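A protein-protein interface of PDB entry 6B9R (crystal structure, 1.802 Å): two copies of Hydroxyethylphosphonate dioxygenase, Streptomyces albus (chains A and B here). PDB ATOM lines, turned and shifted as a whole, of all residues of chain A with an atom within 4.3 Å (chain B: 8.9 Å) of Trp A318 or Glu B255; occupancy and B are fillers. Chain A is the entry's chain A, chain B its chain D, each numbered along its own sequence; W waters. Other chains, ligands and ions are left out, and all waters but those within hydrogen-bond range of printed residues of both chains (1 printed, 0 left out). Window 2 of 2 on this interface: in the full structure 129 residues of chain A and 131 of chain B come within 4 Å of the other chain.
O of Trp A318 is in hydrogen-bond range of N of Phe A330 (2.7 Å). N of Glu B255 sits at hydrogen-bond distance from OG1 of Thr B252 (3.0 Å). NE of Arg B249 is in hydrogen-bond range of O of Leu B289 (2.8 Å). OE1 of Glu B255 lies within salt-bridge range of NE of Arg B259, at 2.7 Å. NH1 of Arg B259 lies within hydrogen-bond range of O of Ala B288 (3.0 Å). The backbone NH (N) of Gln A332 sits at hydrogen-bond distance from the backbone carbonyl oxygen (O) of Ser A316.
Trp A318 touches just these residues of chain B: Arg B249, Leu B250, Glu B255 and Arg B259. Printed residues of chain B within 4 Å of Phe A330: Leu B250. Of the printed residues of chain B, Gln A332 touches Arg B259. Printed residues of chain B within 4 Å of Leu A345: Leu B250 (3.7 Å). Of the printed residues of chain A, Arg B249 touches Trp A318 (3.4 Å). Of the printed residues of chain A, Leu B250 touches Trp A318, Phe A330 and Leu A345. Of chain A, only Trp A318 comes within 4 Å of Glu B255. The nearest residue of chain B that does not touch Trp A318 is Thr B251 (4.2 Å). The nearest printed residue of chain B that does not touch Gln A332 is Ala B288 (5.5 Å).
Among the printed residues, pairs that only touch across the chains: Trp A318 with Arg B249, Trp A318 with Glu B255, Trp A318 with Arg B259, Phe A330 with Leu B250, Gln A332 with Arg B259 and Leu A345 with Leu B250.
Along chain A the printed residues that touch a printed residue of chain B span positions 318 to 345. Hydrophobic or aromatic side chains of chain B within 4 Å of the printed part of chain A: Leu B250. Among the printed residues, no Asp or Glu carboxylate lies within 4 Å of a Lys or Arg side-chain nitrogen of the other chain.
No position is printed for both chains.
Water W1 bridges O of Ser A319 (2.5 Å) and OG1 of Thr B252 (3.4 Å).
The indole nitrogen (NE1) of Trp A318 lies within hydrogen-bond range of the backbone carbonyl oxygen (O) of Leu B250.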
ATOM      1  N   SER A 316      30.568 -28.244 -16.485  1.00  0.00           N
ATOM      2  CA  SER A 316      29.720 -27.493 -17.412  1.00  0.00           C
ATOM      3  C   SER A 316      30.518 -27.051 -18.631  1.00  0.00           C
ATOM      4  O   SER A 316      31.668 -26.619 -18.517  1.00  0.00           O
ATOM      5  CB  SER A 316      29.127 -26.255 -16.727  1.00  0.00           C
ATOM      6  OG  SER A 316      28.124 -26.587 -15.783  1.00  0.00           O
ATOM      7  N   ARG A 317      29.895 -27.137 -19.811  1.00  0.00           N
ATOM      8  CA  ARG A 317      30.550 -26.765 -21.061  1.00  0.00           C
ATOM      9  C   ARG A 317      29.633 -25.872 -21.873  1.00  0.00           C
ATOM     10  O   ARG A 317      28.422 -26.108 -21.928  1.00  0.00           O
ATOM     11  CB  ARG A 317      30.918 -27.997 -21.890  1.00  0.00           C
ATOM     12  CG  ARG A 317      32.082 -28.791 -21.334  1.00  0.00           C
ATOM     13  CD  ARG A 317      32.155 -30.151 -22.020  1.00  0.00           C
ATOM     14  NE  ARG A 317      33.341 -30.876 -21.590  1.00  0.00           N
ATOM     15  CZ  ARG A 317      33.368 -31.697 -20.546  1.00  0.00           C
ATOM     16  NH1 ARG A 317      32.272 -31.893 -19.837  1.00  0.00           N
ATOM     17  NH2 ARG A 317      34.490 -32.322 -20.211  1.00  0.00           N
ATOM     18  N   TRP A 318      30.203 -24.838 -22.494  1.00  0.00           N
ATOM     19  CA  TRP A 318      29.416 -23.974 -23.361  1.00  0.00           C
ATOM     20  C   TRP A 318      30.348 -23.264 -24.330  1.00  0.00           C
ATOM     21  O   TRP A 318      31.571 -23.273 -24.174  1.00  0.00           O
ATOM     22  CB  TRP A 318      28.573 -22.969 -22.561  1.00  0.00           C
ATOM     23  CG  TRP A 318      29.343 -21.891 -21.843  1.00  0.00           C
ATOM     24  CD1 TRP A 318      29.433 -20.578 -22.206  1.00  0.00           C
ATOM     25  CD2 TRP A 318      30.100 -22.025 -20.628  1.00  0.00           C
ATOM     26  NE1 TRP A 318      30.204 -19.890 -21.299  1.00  0.00           N
ATOM     27  CE2 TRP A 318      30.631 -20.756 -20.326  1.00  0.00           C
ATOM     28  CE3 TRP A 318      30.400 -23.101 -19.783  1.00  0.00           C
ATOM     29  CZ2 TRP A 318      31.434 -20.523 -19.203  1.00  0.00           C
ATOM     30  CZ3 TRP A 318      31.194 -22.880 -18.672  1.00  0.00           C
ATOM     31  CH2 TRP A 318      31.706 -21.587 -18.388  1.00  0.00           C
ATOM     32  N   SER A 319      29.744 -22.668 -25.349  1.00  0.00           N
ATOM     33  CA  SER A 319      30.460 -22.066 -26.463  1.00  0.00           C
ATOM     34  C   SER A 319      30.310 -20.554 -26.430  1.00  0.00           C
ATOM     35  O   SER A 319      29.313 -20.019 -25.939  1.00  0.00           O
ATOM     36  CB  SER A 319      29.945 -22.595 -27.799  1.00  0.00           C
ATOM     37  OG  SER A 319      30.396 -23.906 -28.001  1.00  0.00           O
ATOM     38  N   TYR A 328      35.209 -20.033 -29.078  1.00  0.00           N
ATOM     39  CA  TYR A 328      35.832 -20.720 -27.960  1.00  0.00           C
ATOM     40  C   TYR A 328      34.828 -21.695 -27.384  1.00  0.00           C
ATOM     41  O   TYR A 328      33.617 -21.460 -27.438  1.00  0.00           O
ATOM     42  CB  TYR A 328      36.257 -19.753 -26.824  1.00  0.00           C
ATOM     43  CG  TYR A 328      36.915 -18.489 -27.305  1.00  0.00           C
ATOM     44  CD1 TYR A 328      38.136 -18.529 -27.958  1.00  0.00           C
ATOM     45  CD2 TYR A 328      36.316 -17.252 -27.101  1.00  0.00           C
ATOM     46  CE1 TYR A 328      38.741 -17.361 -28.409  1.00  0.00           C
ATOM     47  CE2 TYR A 328      36.916 -16.083 -27.528  1.00  0.00           C
ATOM     48  CZ  TYR A 328      38.131 -16.143 -28.170  1.00  0.00           C
ATOM     49  OH  TYR A 328      38.723 -14.988 -28.606  1.00  0.00           O
ATOM     50  N   ARG A 329      35.334 -22.771 -26.796  1.00  0.00           N
ATOM     51  CA  ARG A 329      34.500 -23.666 -26.004  1.00  0.00           C
ATOM     52  C   ARG A 329      35.074 -23.669 -24.598  1.00  0.00           C
ATOM     53  O   ARG A 329      36.259 -23.966 -24.410  1.00  0.00           O
ATOM     54  CB  ARG A 329      34.456 -25.077 -26.599  1.00  0.00           C
ATOM     55  CG  ARG A 329      33.247 -25.899 -26.131  1.00  0.00           C
ATOM     56  CD  ARG A 329      33.489 -26.522 -24.762  1.00  0.00           C
ATOM     57  NE  ARG A 329      34.638 -27.426 -24.796  1.00  0.00           N
ATOM     58  CZ  ARG A 329      34.593 -28.712 -25.132  1.00  0.00           C
ATOM     59  NH1 ARG A 329      33.440 -29.303 -25.467  1.00  0.00           N
ATOM     60  NH2 ARG A 329      35.713 -29.422 -25.125  1.00  0.00           N
ATOM     61  N   PHE A 330      34.255 -23.299 -23.623  1.00  0.00           N
ATOM     62  CA  PHE A 330      34.708 -23.203 -22.245  1.00  0.00           C
ATOM     63  C   PHE A 330      34.259 -24.420 -21.452  1.00  0.00           C
ATOM     64  O   PHE A 330      33.159 -24.936 -21.669  1.00  0.00           O
ATOM     65  CB  PHE A 330      34.167 -21.952 -21.559  1.00  0.00           C
ATOM     66  CG  PHE A 330      34.582 -20.655 -22.193  1.00  0.00           C
ATOM     67  CD1 PHE A 330      35.921 -20.316 -22.336  1.00  0.00           C
ATOM     68  CD2 PHE A 330      33.623 -19.738 -22.589  1.00  0.00           C
ATOM     69  CE1 PHE A 330      36.289 -19.088 -22.897  1.00  0.00           C
ATOM     70  CE2 PHE A 330      33.988 -18.516 -23.146  1.00  0.00           C
ATOM     71  CZ  PHE A 330      35.323 -18.200 -23.304  1.00  0.00           C
ATOM     72  N   GLN A 332      34.006 -25.337 -17.273  1.00  0.00           N
ATOM     73  CA  GLN A 332      34.098 -24.742 -15.940  1.00  0.00           C
ATOM     74  C   GLN A 332      34.854 -25.678 -15.004  1.00  0.00           C
ATOM     75  O   GLN A 332      34.471 -26.843 -14.836  1.00  0.00           O
ATOM     76  CB  GLN A 332      32.699 -24.445 -15.396  1.00  0.00           C
ATOM     77  CG  GLN A 332      32.659 -23.992 -13.924  1.00  0.00           C
ATOM     78  CD  GLN A 332      31.240 -23.984 -13.346  1.00  0.00           C
ATOM     79  OE1 GLN A 332      30.292 -23.541 -13.998  1.00  0.00           O
ATOM     80  NE2 GLN A 332      31.092 -24.492 -12.120  1.00  0.00           N
ATOM     81  N   LEU A 345      38.790 -21.920 -15.945  1.00  0.00           N
ATOM     82  CA  LEU A 345      38.273 -22.417 -17.211  1.00  0.00           C
ATOM     83  C   LEU A 345      39.329 -23.171 -17.999  1.00  0.00           C
ATOM     84  O   LEU A 345      40.493 -22.765 -18.053  1.00  0.00           O
ATOM     85  CB  LEU A 345      37.754 -21.277 -18.093  1.00  0.00           C
ATOM     86  CG  LEU A 345      36.588 -20.470 -17.525  1.00  0.00           C
ATOM     87  CD1 LEU A 345      36.395 -19.181 -18.334  1.00  0.00           C
ATOM     88  CD2 LEU A 345      35.327 -21.303 -17.532  1.00  0.00           C
ATOM     89  N   MET B 246      28.545 -11.741 -14.932  1.00  0.00           N
ATOM     90  CA  MET B 246      28.475 -12.451 -16.211  1.00  0.00           C
ATOM     91  C   MET B 246      29.799 -12.381 -16.955  1.00  0.00           C
ATOM     92  O   MET B 246      30.269 -13.388 -17.496  1.00  0.00           O
ATOM     93  CB  MET B 246      27.364 -11.868 -17.089  1.00  0.00           C
ATOM     94  CG  MET B 246      25.960 -12.129 -16.573  1.00  0.00           C
ATOM     95  SD  MET B 246      24.749 -11.229 -17.552  1.00  0.00           S
ATOM     96  CE  MET B 246      24.848 -12.137 -19.112  1.00  0.00           C
ATOM     97  N   ALA B 247      30.415 -11.197 -17.001  1.00  0.00           N
ATOM     98  CA  ALA B 247      31.698 -11.064 -17.679  1.00  0.00           C
ATOM     99  C   ALA B 247      32.784 -11.857 -16.966  1.00  0.00           C
ATOM    100  O   ALA B 247      33.679 -12.415 -17.618  1.00  0.00           O
ATOM    101  CB  ALA B 247      32.093  -9.584 -17.779  1.00  0.00           C
ATOM    102  N   ALA B 248      32.720 -11.920 -15.634  1.00  0.00           N
ATOM    103  CA  ALA B 248      33.692 -12.711 -14.886  1.00  0.00           C
ATOM    104  C   ALA B 248      33.540 -14.202 -15.171  1.00  0.00           C
ATOM    105  O   ALA B 248      34.530 -14.944 -15.137  1.00  0.00           O
ATOM    106  CB  ALA B 248      33.550 -12.444 -13.389  1.00  0.00           C
ATOM    107  N   ARG B 249      32.317 -14.656 -15.440  1.00  0.00           N
ATOM    108  CA  ARG B 249      32.069 -16.072 -15.701  1.00  0.00           C
ATOM    109  C   ARG B 249      32.098 -16.424 -17.180  1.00  0.00           C
ATOM    110  O   ARG B 249      32.052 -17.613 -17.516  1.00  0.00           O
ATOM    111  CB  ARG B 249      30.714 -16.487 -15.122  1.00  0.00           C
ATOM    112  CG  ARG B 249      30.665 -16.494 -13.597  1.00  0.00           C
ATOM    113  CD  ARG B 249      31.672 -17.476 -13.035  1.00  0.00           C
ATOM    114  NE  ARG B 249      31.392 -17.702 -11.630  1.00  0.00           N
ATOM    115  CZ  ARG B 249      32.086 -17.167 -10.636  1.00  0.00           C
ATOM    116  NH1 ARG B 249      33.136 -16.393 -10.895  1.00  0.00           N
ATOM    117  NH2 ARG B 249      31.731 -17.419  -9.385  1.00  0.00           N
ATOM    118  N   LEU B 250      32.174 -15.428 -18.062  1.00  0.00           N
ATOM    119  CA  LEU B 250      32.127 -15.634 -19.506  1.00  0.00           C
ATOM    120  C   LEU B 250      30.837 -16.331 -19.925  1.00  0.00           C
ATOM    121  O   LEU B 250      30.817 -17.131 -20.865  1.00  0.00           O
ATOM    122  CB  LEU B 250      33.373 -16.385 -19.999  1.00  0.00           C
ATOM    123  CG  LEU B 250      34.560 -15.413 -20.148  1.00  0.00           C
ATOM    124  CD1 LEU B 250      35.932 -16.090 -20.221  1.00  0.00           C
ATOM    125  CD2 LEU B 250      34.352 -14.556 -21.371  1.00  0.00           C
ATOM    126  N   THR B 251      29.751 -16.010 -19.230  1.00  0.00           N
ATOM    127  CA  THR B 251      28.417 -16.431 -19.625  1.00  0.00           C
ATOM    128  C   THR B 251      27.778 -15.344 -20.472  1.00  0.00           C
ATOM    129  O   THR B 251      27.669 -14.190 -20.038  1.00  0.00           O
ATOM    130  CB  THR B 251      27.526 -16.702 -18.409  1.00  0.00           C
ATOM    131  OG1 THR B 251      27.482 -15.534 -17.567  1.00  0.00           O
ATOM    132  CG2 THR B 251      28.016 -17.909 -17.610  1.00  0.00           C
ATOM    133  N   THR B 252      27.333 -15.711 -21.666  1.00  0.00           N
ATOM    134  CA  THR B 252      26.502 -14.797 -22.427  1.00  0.00           C
ATOM    135  C   THR B 252      25.120 -14.694 -21.780  1.00  0.00           C
ATOM    136  O   THR B 252      24.751 -15.485 -20.913  1.00  0.00           O
ATOM    137  CB  THR B 252      26.348 -15.285 -23.864  1.00  0.00           C
ATOM    138  OG1 THR B 252      25.744 -16.578 -23.838  1.00  0.00           O
ATOM    139  CG2 THR B 252      27.696 -15.387 -24.553  1.00  0.00           C
ATOM    140  N   VAL B 253      24.357 -13.688 -22.210  1.00  0.00           N
ATOM    141  CA  VAL B 253      22.940 -13.610 -21.854  1.00  0.00           C
ATOM    142  C   VAL B 253      22.245 -14.941 -22.137  1.00  0.00           C
ATOM    143  O   VAL B 253      21.499 -15.463 -21.300  1.00  0.00           O
ATOM    144  CB  VAL B 253      22.271 -12.448 -22.608  1.00  0.00           C
ATOM    145  CG1 VAL B 253      20.767 -12.585 -22.593  1.00  0.00           C
ATOM    146  CG2 VAL B 253      22.695 -11.110 -21.977  1.00  0.00           C
ATOM    147  N   THR B 254      22.500 -15.522 -23.312  1.00  0.00           N
ATOM    148  CA  THR B 254      21.815 -16.763 -23.673  1.00  0.00           C
ATOM    149  C   THR B 254      22.233 -17.918 -22.763  1.00  0.00           C
ATOM    150  O   THR B 254      21.382 -18.699 -22.323  1.00  0.00           O
ATOM    151  CB  THR B 254      22.064 -17.098 -25.144  1.00  0.00           C
ATOM    152  OG1 THR B 254      21.674 -15.981 -25.951  1.00  0.00           O
ATOM    153  CG2 THR B 254      21.235 -18.295 -25.570  1.00  0.00           C
ATOM    154  N   GLU B 255      23.533 -18.043 -22.455  1.00  0.00           N
ATOM    155  CA  GLU B 255      23.963 -19.144 -21.593  1.00  0.00           C
ATOM    156  C   GLU B 255      23.437 -18.974 -20.175  1.00  0.00           C
ATOM    157  O   GLU B 255      23.072 -19.957 -19.522  1.00  0.00           O
ATOM    158  CB  GLU B 255      25.496 -19.275 -21.578  1.00  0.00           C
ATOM    159  CG  GLU B 255      26.071 -20.246 -20.501  1.00  0.00           C
ATOM    160  CD  GLU B 255      25.699 -21.723 -20.700  1.00  0.00           C
ATOM    161  OE1 GLU B 255      25.898 -22.536 -19.759  1.00  0.00           O
ATOM    162  OE2 GLU B 255      25.223 -22.080 -21.790  1.00  0.00           O
ATOM    163  N   LEU B 256      23.419 -17.740 -19.662  1.00  0.00           N
ATOM    164  CA  LEU B 256      22.892 -17.527 -18.316  1.00  0.00           C
ATOM    165  C   LEU B 256      21.386 -17.766 -18.265  1.00  0.00           C
ATOM    166  O   LEU B 256      20.868 -18.303 -17.276  1.00  0.00           O
ATOM    167  CB  LEU B 256      23.220 -16.113 -17.847  1.00  0.00           C
ATOM    168  CG  LEU B 256      22.685 -15.752 -16.462  1.00  0.00           C
ATOM    169  CD1 LEU B 256      23.090 -16.767 -15.388  1.00  0.00           C
ATOM    170  CD2 LEU B 256      23.189 -14.343 -16.113  1.00  0.00           C
ATOM    171  N   ALA B 257      20.663 -17.338 -19.298  1.00  0.00           N
ATOM    172  CA  ALA B 257      19.257 -17.720 -19.416  1.00  0.00           C
ATOM    173  C   ALA B 257      19.112 -19.238 -19.434  1.00  0.00           C
ATOM    174  O   ALA B 257      18.285 -19.803 -18.709  1.00  0.00           O
ATOM    175  CB  ALA B 257      18.654 -17.102 -20.677  1.00  0.00           C
ATOM    176  N   ASP B 258      19.924 -19.910 -20.253  1.00  0.00           N
ATOM    177  CA  ASP B 258      19.896 -21.374 -20.361  1.00  0.00           C
ATOM    178  C   ASP B 258      20.033 -22.032 -18.984  1.00  0.00           C
ATOM    179  O   ASP B 258      19.256 -22.925 -18.625  1.00  0.00           O
ATOM    180  CB  ASP B 258      21.037 -21.812 -21.295  1.00  0.00           C
ATOM    181  CG  ASP B 258      20.775 -23.144 -22.010  1.00  0.00           C
ATOM    182  OD1 ASP B 258      19.660 -23.688 -21.927  1.00  0.00           O
ATOM    183  OD2 ASP B 258      21.720 -23.638 -22.666  1.00  0.00           O
ATOM    184  N   ARG B 259      21.016 -21.580 -18.191  1.00  0.00           N
ATOM    185  CA  ARG B 259      21.286 -22.194 -16.891  1.00  0.00           C
ATOM    186  C   ARG B 259      20.204 -21.877 -15.872  1.00  0.00           C
ATOM    187  O   ARG B 259      19.865 -22.715 -15.033  1.00  0.00           O
ATOM    188  CB  ARG B 259      22.625 -21.712 -16.341  1.00  0.00           C
ATOM    189  CG  ARG B 259      23.834 -22.123 -17.134  1.00  0.00           C
ATOM    190  CD  ARG B 259      25.071 -21.631 -16.401  1.00  0.00           C
ATOM    191  NE  ARG B 259      26.275 -21.800 -17.197  1.00  0.00           N
ATOM    192  CZ  ARG B 259      27.490 -21.500 -16.756  1.00  0.00           C
ATOM    193  NH1 ARG B 259      27.659 -21.037 -15.515  1.00  0.00           N
ATOM    194  NH2 ARG B 259      28.535 -21.676 -17.547  1.00  0.00           N
ATOM    195  N   SER B 260      19.695 -20.653 -15.882  1.00  0.00           N
ATOM    196  CA  SER B 260      18.880 -20.195 -14.769  1.00  0.00           C
ATOM    197  C   SER B 260      17.398 -20.438 -14.977  1.00  0.00           C
ATOM    198  O   SER B 260      16.625 -20.349 -14.012  1.00  0.00           O
ATOM    199  CB  SER B 260      19.117 -18.695 -14.541  1.00  0.00           C
ATOM    200  OG  SER B 260      18.630 -18.002 -15.675  1.00  0.00           O
ATOM    201  N   GLY B 261      16.974 -20.710 -16.206  1.00  0.00           N
ATOM    202  CA  GLY B 261      15.561 -20.844 -16.478  1.00  0.00           C
ATOM    203  C   GLY B 261      14.849 -19.548 -16.800  1.00  0.00           C
ATOM    204  O   GLY B 261      13.652 -19.581 -17.114  1.00  0.00           O
ATOM    205  N   LEU B 262      15.531 -18.409 -16.720  1.00  0.00           N
ATOM    206  CA  LEU B 262      14.935 -17.157 -17.153  1.00  0.00           C
ATOM    207  C   LEU B 262      15.020 -17.046 -18.668  1.00  0.00           C
ATOM    208  O   LEU B 262      15.956 -17.550 -19.285  1.00  0.00           O
ATOM    209  CB  LEU B 262      15.641 -15.957 -16.507  1.00  0.00           C
ATOM    210  CG  LEU B 262      15.368 -15.602 -15.041  1.00  0.00           C
ATOM    211  CD1 LEU B 262      15.929 -16.624 -14.088  1.00  0.00           C
ATOM    212  CD2 LEU B 262      15.949 -14.231 -14.718  1.00  0.00           C
ATOM    213  N   LYS B 263      14.017 -16.398 -19.265  1.00  0.00           N
ATOM    214  CA  LYS B 263      14.025 -16.175 -20.706  1.00  0.00           C
ATOM    215  C   LYS B 263      15.223 -15.325 -21.107  1.00  0.00           C
ATOM    216  O   LYS B 263      15.635 -14.418 -20.377  1.00  0.00           O
ATOM    217  CB  LYS B 263      12.738 -15.470 -21.144  1.00  0.00           C
ATOM    218  CG  LYS B 263      11.473 -16.290 -20.886  1.00  0.00           C
ATOM    219  CD  LYS B 263      10.200 -15.460 -20.970  1.00  0.00           C
ATOM    220  CE  LYS B 263       9.672 -15.364 -22.386  1.00  0.00           C
ATOM    221  NZ  LYS B 263      10.508 -14.478 -23.239  1.00  0.00           N
ATOM    222  N   THR B 264      15.764 -15.612 -22.297  1.00  0.00           N
ATOM    223  CA  THR B 264      16.880 -14.828 -22.829  1.00  0.00           C
ATOM    224  C   THR B 264      16.572 -13.336 -22.787  1.00  0.00           C
ATOM    225  O   THR B 264      17.395 -12.525 -22.340  1.00  0.00           O
ATOM    226  CB  THR B 264      17.195 -15.254 -24.266  1.00  0.00           C
ATOM    227  OG1 THR B 264      17.534 -16.645 -24.301  1.00  0.00           O
ATOM    228  CG2 THR B 264      18.364 -14.446 -24.812  1.00  0.00           C
ATOM    229  N   VAL B 267      16.899 -11.906 -19.142  1.00  0.00           N
ATOM    230  CA  VAL B 267      18.274 -11.710 -18.692  1.00  0.00           C
ATOM    231  C   VAL B 267      18.871 -10.480 -19.362  1.00  0.00           C
ATOM    232  O   VAL B 267      19.508  -9.649 -18.708  1.00  0.00           O
ATOM    233  CB  VAL B 267      19.123 -12.962 -18.970  1.00  0.00           C
ATOM    234  CG1 VAL B 267      20.553 -12.706 -18.557  1.00  0.00           C
ATOM    235  CG2 VAL B 267      18.544 -14.187 -18.222  1.00  0.00           C
ATOM    236  N   LEU B 285      19.657 -16.801 -10.832  1.00  0.00           N
ATOM    237  CA  LEU B 285      20.843 -16.254 -11.490  1.00  0.00           C
ATOM    238  C   LEU B 285      22.099 -16.522 -10.675  1.00  0.00           C
ATOM    239  O   LEU B 285      23.136 -16.925 -11.218  1.00  0.00           O
ATOM    240  CB  LEU B 285      20.656 -14.750 -11.718  1.00  0.00           C
ATOM    241  CG  LEU B 285      19.559 -14.375 -12.728  1.00  0.00           C
ATOM    242  CD1 LEU B 285      19.229 -12.890 -12.630  1.00  0.00           C
ATOM    243  CD2 LEU B 285      19.998 -14.756 -14.151  1.00  0.00           C
ATOM    244  N   ALA B 288      23.155 -20.063 -10.928  1.00  0.00           N
ATOM    245  CA  ALA B 288      23.747 -20.332 -12.237  1.00  0.00           C
ATOM    246  C   ALA B 288      25.145 -19.758 -12.382  1.00  0.00           C
ATOM    247  O   ALA B 288      25.906 -20.235 -13.227  1.00  0.00           O
ATOM    248  CB  ALA B 288      22.854 -19.781 -13.354  1.00  0.00           C
ATOM    249  N   LEU B 289      25.494 -18.739 -11.592  1.00  0.00           N
ATOM    250  CA  LEU B 289      26.786 -18.070 -11.689  1.00  0.00           C
ATOM    251  C   LEU B 289      27.763 -18.507 -10.610  1.00  0.00           C
ATOM    252  O   LEU B 289      28.873 -17.959 -10.533  1.00  0.00           O
ATOM    253  CB  LEU B 289      26.595 -16.548 -11.634  1.00  0.00           C
ATOM    254  CG  LEU B 289      25.822 -15.986 -12.829  1.00  0.00           C
ATOM    255  CD1 LEU B 289      25.343 -14.568 -12.542  1.00  0.00           C
ATOM    256  CD2 LEU B 289      26.690 -16.023 -14.091  1.00  0.00           C
HETATM  257  O   HOH W   1      27.053 -19.517 -24.957  1.00  0.00           O
